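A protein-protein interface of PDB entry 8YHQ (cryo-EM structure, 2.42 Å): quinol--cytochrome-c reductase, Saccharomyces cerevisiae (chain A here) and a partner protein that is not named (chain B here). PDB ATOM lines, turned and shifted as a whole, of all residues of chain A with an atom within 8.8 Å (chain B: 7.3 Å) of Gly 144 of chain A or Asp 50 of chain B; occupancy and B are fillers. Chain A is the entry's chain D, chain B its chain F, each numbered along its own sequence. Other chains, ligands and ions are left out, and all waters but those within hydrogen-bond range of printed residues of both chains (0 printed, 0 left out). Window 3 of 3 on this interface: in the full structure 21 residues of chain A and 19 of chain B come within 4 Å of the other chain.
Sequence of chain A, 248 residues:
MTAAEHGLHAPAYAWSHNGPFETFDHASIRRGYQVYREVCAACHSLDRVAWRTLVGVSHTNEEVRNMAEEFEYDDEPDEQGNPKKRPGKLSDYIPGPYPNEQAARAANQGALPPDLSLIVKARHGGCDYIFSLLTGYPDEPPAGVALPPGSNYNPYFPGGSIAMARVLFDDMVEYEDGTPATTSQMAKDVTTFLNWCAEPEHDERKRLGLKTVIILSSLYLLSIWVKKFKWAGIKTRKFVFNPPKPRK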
ATOM      1  N   ALA A   4      -4.067  13.864  21.009  1.00  0.00           N
ATOM      2  CA  ALA A   4      -4.303  12.454  20.718  1.00  0.00           C
ATOM      3  C   ALA A   4      -5.771  12.190  20.413  1.00  0.00           C
ATOM      4  O   ALA A   4      -6.100  11.505  19.439  1.00  0.00           O
ATOM      5  CB  ALA A   4      -3.832  11.592  21.884  1.00  0.00           C
ATOM      6  N   PRO A 141       3.691   0.609  19.493  1.00  0.00           N
ATOM      7  CA  PRO A 141       2.993   1.785  19.997  1.00  0.00           C
ATOM      8  C   PRO A 141       3.867   2.531  20.987  1.00  0.00           C
ATOM      9  O   PRO A 141       4.788   1.939  21.571  1.00  0.00           O
ATOM     10  CB  PRO A 141       1.744   1.201  20.672  1.00  0.00           C
ATOM     11  CG  PRO A 141       2.086  -0.187  20.966  1.00  0.00           C
ATOM     12  CD  PRO A 141       2.971  -0.622  19.859  1.00  0.00           C
ATOM     13  N   PRO A 142       3.630   3.825  21.199  1.00  0.00           N
ATOM     14  CA  PRO A 142       4.488   4.575  22.119  1.00  0.00           C
ATOM     15  C   PRO A 142       4.326   4.077  23.545  1.00  0.00           C
ATOM     16  O   PRO A 142       3.237   3.693  23.970  1.00  0.00           O
ATOM     17  CB  PRO A 142       4.007   6.020  21.955  1.00  0.00           C
ATOM     18  CG  PRO A 142       2.658   5.917  21.432  1.00  0.00           C
ATOM     19  CD  PRO A 142       2.587   4.683  20.617  1.00  0.00           C
ATOM     20  N   ALA A 143       5.432   4.082  24.278  1.00  0.00           N
ATOM     21  CA  ALA A 143       5.489   3.446  25.588  1.00  0.00           C
ATOM     22  C   ALA A 143       4.561   4.165  26.553  1.00  0.00           C
ATOM     23  O   ALA A 143       4.747   5.352  26.834  1.00  0.00           O
ATOM     24  CB  ALA A 143       6.923   3.450  26.102  1.00  0.00           C
ATOM     25  N   GLY A 144       3.555   3.445  27.051  1.00  0.00           N
ATOM     26  CA  GLY A 144       2.619   3.971  28.026  1.00  0.00           C
ATOM     27  C   GLY A 144       1.182   3.735  27.650  1.00  0.00           C
ATOM     28  O   GLY A 144       0.328   3.493  28.509  1.00  0.00           O
ATOM     29  N   VAL A 145       0.898   3.827  26.364  1.00  0.00           N
ATOM     30  CA  VAL A 145      -0.460   3.637  25.877  1.00  0.00           C
ATOM     31  C   VAL A 145      -0.849   2.176  26.052  1.00  0.00           C
ATOM     32  O   VAL A 145      -0.104   1.265  25.668  1.00  0.00           O
ATOM     33  CB  VAL A 145      -0.580   4.108  24.412  1.00  0.00           C
ATOM     34  CG1 VAL A 145       0.185   3.199  23.480  1.00  0.00           C
ATOM     35  CG2 VAL A 145      -2.036   4.188  23.989  1.00  0.00           C
ATOM     36  N   ALA A 146      -2.013   1.951  26.656  1.00  0.00           N
ATOM     37  CA  ALA A 146      -2.525   0.615  26.918  1.00  0.00           C
ATOM     38  C   ALA A 146      -3.650   0.346  25.912  1.00  0.00           C
ATOM     39  O   ALA A 146      -4.763   0.873  26.048  1.00  0.00           O
ATOM     40  CB  ALA A 146      -3.047   0.498  28.338  1.00  0.00           C
ATOM     41  N   LEU A 147      -3.366  -0.460  24.890  1.00  0.00           N
ATOM     42  CA  LEU A 147      -4.364  -0.820  23.913  1.00  0.00           C
ATOM     43  C   LEU A 147      -5.248  -1.941  24.452  1.00  0.00           C
ATOM     44  O   LEU A 147      -4.760  -2.818  25.138  1.00  0.00           O
ATOM     45  CB  LEU A 147      -3.693  -1.254  22.615  1.00  0.00           C
ATOM     46  CG  LEU A 147      -2.917  -0.243  21.766  1.00  0.00           C
ATOM     47  CD1 LEU A 147      -2.307  -0.912  20.582  1.00  0.00           C
ATOM     48  CD2 LEU A 147      -3.819   0.871  21.325  1.00  0.00           C
ATOM     49  N   TYR A 153      -2.669   0.464  16.948  1.00  0.00           N
ATOM     50  CA  TYR A 153      -2.320   1.868  17.114  1.00  0.00           C
ATOM     51  C   TYR A 153      -1.817   2.466  15.806  1.00  0.00           C
ATOM     52  O   TYR A 153      -0.921   1.908  15.164  1.00  0.00           O
ATOM     53  CB  TYR A 153      -1.248   2.031  18.192  1.00  0.00           C
ATOM     54  CG  TYR A 153      -0.870   3.465  18.473  1.00  0.00           C
ATOM     55  CD1 TYR A 153      -1.573   4.222  19.390  1.00  0.00           C
ATOM     56  CD2 TYR A 153       0.197   4.057  17.825  1.00  0.00           C
ATOM     57  CE1 TYR A 153      -1.228   5.527  19.643  1.00  0.00           C
ATOM     58  CE2 TYR A 153       0.543   5.360  18.068  1.00  0.00           C
ATOM     59  CZ  TYR A 153      -0.168   6.089  18.982  1.00  0.00           C
ATOM     60  OH  TYR A 153       0.184   7.390  19.230  1.00  0.00           O
ATOM     61  N   GLY A 159      -8.221   9.309  18.739  1.00  0.00           N
ATOM     62  CA  GLY A 159      -8.167   8.438  19.896  1.00  0.00           C
ATOM     63  C   GLY A 159      -6.868   7.666  19.977  1.00  0.00           C
ATOM     64  O   GLY A 159      -6.303   7.496  21.060  1.00  0.00           O
ATOM     65  N   TYR B  26      11.884  11.922  23.043  1.00  0.00           N
ATOM     66  CA  TYR B  26      10.868  10.874  23.021  1.00  0.00           C
ATOM     67  C   TYR B  26      11.335   9.652  23.798  1.00  0.00           C
ATOM     68  O   TYR B  26      10.537   8.981  24.463  1.00  0.00           O
ATOM     69  CB  TYR B  26      10.531  10.479  21.586  1.00  0.00           C
ATOM     70  CG  TYR B  26       9.808   9.160  21.518  1.00  0.00           C
ATOM     71  CD1 TYR B  26       8.487   9.053  21.914  1.00  0.00           C
ATOM     72  CD2 TYR B  26      10.455   8.013  21.090  1.00  0.00           C
ATOM     73  CE1 TYR B  26       7.829   7.855  21.870  1.00  0.00           C
ATOM     74  CE2 TYR B  26       9.806   6.810  21.046  1.00  0.00           C
ATOM     75  CZ  TYR B  26       8.490   6.735  21.433  1.00  0.00           C
ATOM     76  OH  TYR B  26       7.829   5.535  21.395  1.00  0.00           O
ATOM     77  N   CYS B  29      11.889   9.918  27.635  1.00  0.00           N
ATOM     78  CA  CYS B  29      10.574   9.955  28.254  1.00  0.00           C
ATOM     79  C   CYS B  29      10.204   8.487  28.437  1.00  0.00           C
ATOM     80  O   CYS B  29       9.741   8.138  29.503  1.00  0.00           O
ATOM     81  CB  CYS B  29       9.652  10.750  27.334  1.00  0.00           C
ATOM     82  SG  CYS B  29       7.897  10.618  27.743  1.00  0.00           S
ATOM     83  N   ALA B  30      10.447   7.640  27.443  1.00  0.00           N
ATOM     84  CA  ALA B  30      10.021   6.237  27.459  1.00  0.00           C
ATOM     85  C   ALA B  30      10.985   5.385  28.244  1.00  0.00           C
ATOM     86  O   ALA B  30      10.763   4.191  28.370  1.00  0.00           O
ATOM     87  CB  ALA B  30       9.932   5.789  26.038  1.00  0.00           C
ATOM     88  N   VAL B  33       9.208   5.850  31.822  1.00  0.00           N
ATOM     89  CA  VAL B  33       7.927   5.089  31.957  1.00  0.00           C
ATOM     90  C   VAL B  33       8.367   3.624  32.003  1.00  0.00           C
ATOM     91  O   VAL B  33       7.736   2.750  31.428  1.00  0.00           O
ATOM     92  CB  VAL B  33       6.944   5.327  30.794  1.00  0.00           C
ATOM     93  CG1 VAL B  33       5.637   4.571  30.947  1.00  0.00           C
ATOM     94  CG2 VAL B  33       6.669   6.807  30.605  1.00  0.00           C
ATOM     95  N   GLN B  36       9.447   2.886  36.252  1.00  0.00           N
ATOM     96  CA  GLN B  36       8.180   3.274  36.914  1.00  0.00           C
ATOM     97  C   GLN B  36       7.061   2.344  36.447  1.00  0.00           C
ATOM     98  O   GLN B  36       6.018   2.328  37.095  1.00  0.00           O
ATOM     99  CB  GLN B  36       7.904   4.742  36.660  1.00  0.00           C
ATOM    100  CG  GLN B  36       6.795   5.042  35.676  1.00  0.00           C
ATOM    101  CD  GLN B  36       6.075   6.281  36.140  1.00  0.00           C
ATOM    102  OE1 GLN B  36       6.393   7.398  35.740  1.00  0.00           O
ATOM    103  NE2 GLN B  36       5.108   6.086  37.019  1.00  0.00           N
ATOM    104  N   GLN B  37       7.278   1.573  35.396  1.00  0.00           N
ATOM    105  CA  GLN B  37       6.272   0.553  35.021  1.00  0.00           C
ATOM    106  C   GLN B  37       6.461  -0.565  36.032  1.00  0.00           C
ATOM    107  O   GLN B  37       5.487  -1.295  36.249  1.00  0.00           O
ATOM    108  CB  GLN B  37       6.417   0.123  33.563  1.00  0.00           C
ATOM    109  CG  GLN B  37       5.718   1.063  32.587  1.00  0.00           C
ATOM    110  CD  GLN B  37       4.932   0.374  31.499  1.00  0.00           C
ATOM    111  OE1 GLN B  37       4.124  -0.513  31.756  1.00  0.00           O
ATOM    112  NE2 GLN B  37       5.156   0.779  30.263  1.00  0.00           N
ATOM    113  N   TYR B  42       0.383   0.431  40.456  1.00  0.00           N
ATOM    114  CA  TYR B  42       0.257   0.923  39.067  1.00  0.00           C
ATOM    115  C   TYR B  42      -1.017   0.341  38.509  1.00  0.00           C
ATOM    116  O   TYR B  42      -1.785   1.121  37.893  1.00  0.00           O
ATOM    117  CB  TYR B  42       1.460   0.519  38.225  1.00  0.00           C
ATOM    118  CG  TYR B  42       1.647   1.345  36.980  1.00  0.00           C
ATOM    119  CD1 TYR B  42       2.663   2.280  36.891  1.00  0.00           C
ATOM    120  CD2 TYR B  42       0.799   1.192  35.893  1.00  0.00           C
ATOM    121  CE1 TYR B  42       2.824   3.056  35.755  1.00  0.00           C
ATOM    122  CE2 TYR B  42       0.952   1.956  34.752  1.00  0.00           C
ATOM    123  CZ  TYR B  42       1.963   2.895  34.685  1.00  0.00           C
ATOM    124  OH  TYR B  42       2.098   3.639  33.539  1.00  0.00           O
ATOM    125  N   LYS B  48      -1.172   7.813  35.189  1.00  0.00           N
ATOM    126  CA  LYS B  48       0.150   7.292  34.758  1.00  0.00           C
ATOM    127  C   LYS B  48       0.676   8.024  33.505  1.00  0.00           C
ATOM    128  O   LYS B  48      -0.107   8.154  32.536  1.00  0.00           O
ATOM    129  CB  LYS B  48      -0.101   5.808  34.476  1.00  0.00           C
ATOM    130  CG  LYS B  48      -1.518   5.320  34.718  1.00  0.00           C
ATOM    131  CD  LYS B  48      -1.716   3.888  34.301  1.00  0.00           C
ATOM    132  CE  LYS B  48      -2.656   3.130  35.210  1.00  0.00           C
ATOM    133  NZ  LYS B  48      -2.350   1.685  35.192  1.00  0.00           N
ATOM    134  N   GLU B  49       1.912   8.519  33.486  1.00  0.00           N
ATOM    135  CA  GLU B  49       2.380   9.320  32.310  1.00  0.00           C
ATOM    136  C   GLU B  49       2.735   8.480  31.091  1.00  0.00           C
ATOM    137  O   GLU B  49       3.166   7.359  31.278  1.00  0.00           O
ATOM    138  CB  GLU B  49       3.599  10.150  32.626  1.00  0.00           C
ATOM    139  CG  GLU B  49       4.144  10.922  31.451  1.00  0.00           C
ATOM    140  CD  GLU B  49       5.605  11.263  31.648  1.00  0.00           C
ATOM    141  OE1 GLU B  49       6.183  11.908  30.770  1.00  0.00           O
ATOM    142  OE2 GLU B  49       6.146  10.882  32.690  1.00  0.00           O
ATOM    143  N   ASP B  50       2.586   9.022  29.882  1.00  0.00           N
ATOM    144  CA  ASP B  50       2.782   8.292  28.609  1.00  0.00           C
ATOM    145  C   ASP B  50       3.688   9.063  27.681  1.00  0.00           C
ATOM    146  O   ASP B  50       4.339  10.005  28.123  1.00  0.00           O
ATOM    147  CB  ASP B  50       1.534   8.309  27.730  1.00  0.00           C
ATOM    148  CG  ASP B  50       0.354   7.513  28.226  1.00  0.00           C
ATOM    149  OD1 ASP B  50       0.486   6.890  29.290  1.00  0.00           O
ATOM    150  OD2 ASP B  50      -0.683   7.529  27.533  1.00  0.00           O
ATOM    151  N   CYS B  51       3.607   8.712  26.400  1.00  0.00           N
ATOM    152  CA  CYS B  51       4.358   9.528  25.426  1.00  0.00           C
ATOM    153  C   CYS B  51       3.654   9.772  24.061  1.00  0.00           C
ATOM    154  O   CYS B  51       4.420   9.722  23.142  1.00  0.00           O
ATOM    155  CB  CYS B  51       5.724   8.871  25.257  1.00  0.00           C
ATOM    156  SG  CYS B  51       6.616   8.409  26.761  1.00  0.00           S
ATOM    157  N   VAL B  52       2.341  10.094  23.887  1.00  0.00           N
ATOM    158  CA  VAL B  52       1.846  10.454  22.567  1.00  0.00           C
ATOM    159  C   VAL B  52       2.386  11.805  22.116  1.00  0.00           C
ATOM    160  O   VAL B  52       2.481  12.056  20.910  1.00  0.00           O
ATOM    161  CB  VAL B  52       0.308  10.463  22.546  1.00  0.00           C
ATOM    162  CG1 VAL B  52      -0.208  10.667  21.138  1.00  0.00           C
ATOM    163  CG2 VAL B  52      -0.239   9.171  23.124  1.00  0.00           C
ATOM    164  N   GLU B  53       2.762  12.675  23.054  1.00  0.00           N
ATOM    165  CA  GLU B  53       3.105  14.050  22.716  1.00  0.00           C
ATOM    166  C   GLU B  53       4.479  14.131  22.064  1.00  0.00           C
ATOM    167  O   GLU B  53       4.641  14.729  20.995  1.00  0.00           O
ATOM    168  CB  GLU B  53       3.043  14.909  23.979  1.00  0.00           C
ATOM    169  CG  GLU B  53       3.428  16.360  23.791  1.00  0.00           C
ATOM    170  CD  GLU B  53       3.006  17.244  24.951  1.00  0.00           C
ATOM    171  OE1 GLU B  53       3.751  18.193  25.271  1.00  0.00           O
ATOM    172  OE2 GLU B  53       1.929  17.004  25.536  1.00  0.00           O
ATOM    173  N   GLU B  54       5.484  13.530  22.698  1.00  0.00           N
ATOM    174  CA  GLU B  54       6.836  13.547  22.154  1.00  0.00           C
ATOM    175  C   GLU B  54       6.920  12.763  20.852  1.00  0.00           C
ATOM    176  O   GLU B  54       7.711  13.103  19.966  1.00  0.00           O
ATOM    177  CB  GLU B  54       7.817  12.980  23.175  1.00  0.00           C
ATOM    178  CG  GLU B  54       7.965  13.797  24.446  1.00  0.00           C
ATOM    179  CD  GLU B  54       6.905  13.502  25.486  1.00  0.00           C
ATOM    180  OE1 GLU B  54       5.914  12.818  25.156  1.00  0.00           O
ATOM    181  OE2 GLU B  54       7.062  13.955  26.638  1.00  0.00           O
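Among the printed residues, merely in contact across the chains: Pro 142 of chain A with Tyr 26 of chain B (3.6 Å), Ala 143 of chain A with Ala 30 of chain B (3.8 Å), Tyr 153 of chain A with Val 52 of chain B (3.8 Å), Ala 4 of chain A with Val 52 of chain B (3.8 Å), Pro 142 of chain A with Cys 51 of chain B (3.9 Å) and Ala 143 of chain A with Asp 50 of chain B (3.95 Å).
Hydrophobic or aromatic side chains of chain B that line the printed part of chain A: Tyr 26, Ala 30 and Val 52.
Among the printed residues, no Asp or Glu carboxylate lies within 4 Å of a Lys or Arg side-chain nitrogen of the other chain.
The backbone carbonyl oxygen of Ala 143 of chain A lies within hydrogen-bond range of the side-chain sulfur of Cys 51 of chain B, 3.6 Å away.
O of Gly 144 of chain A lies close to OD1 of Asp 50 of chain B, at 3.5 Å.
Of the printed residues of chain B, Gly 144 of chain A touches Asp 50 (3.5 Å).
Printed residues of chain A within 4 Å of Asp 50 of chain B: Ala 143 and Gly 144.
Cys 51 of chain B touches just these residues of chain A: Pro 142 (3.9 Å) and Ala 143 (3.6 Å).
Printed residues of chain B within 4 Å of Pro 142 of chain A: Tyr 26 and Cys 51.
Of the printed residues of chain A, Tyr 26 of chain B touches Pro 142 (3.6 Å).
Printed residues of chain B within 4 Å of Tyr 153 of chain A: Val 52.
The nearest residue of chain B that does not touch Gly 144 of chain A is Val 33 of chain B (4.2 Å).
The nearest printed residue of chain A that does not touch Val 52 of chain B is Pro 142 of chain A (4.7 Å).
The backbone carbonyl oxygen of Ala 4 of chain A lies within hydrogen-bond range of the backbone NH of Gly 159 of chain A (3.1 Å).
The side-chain sulfur (SG) of Cys 29 of chain B sits at hydrogen-bond distance from the backbone carbonyl oxygen (O) of Asp 50 of chain B.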
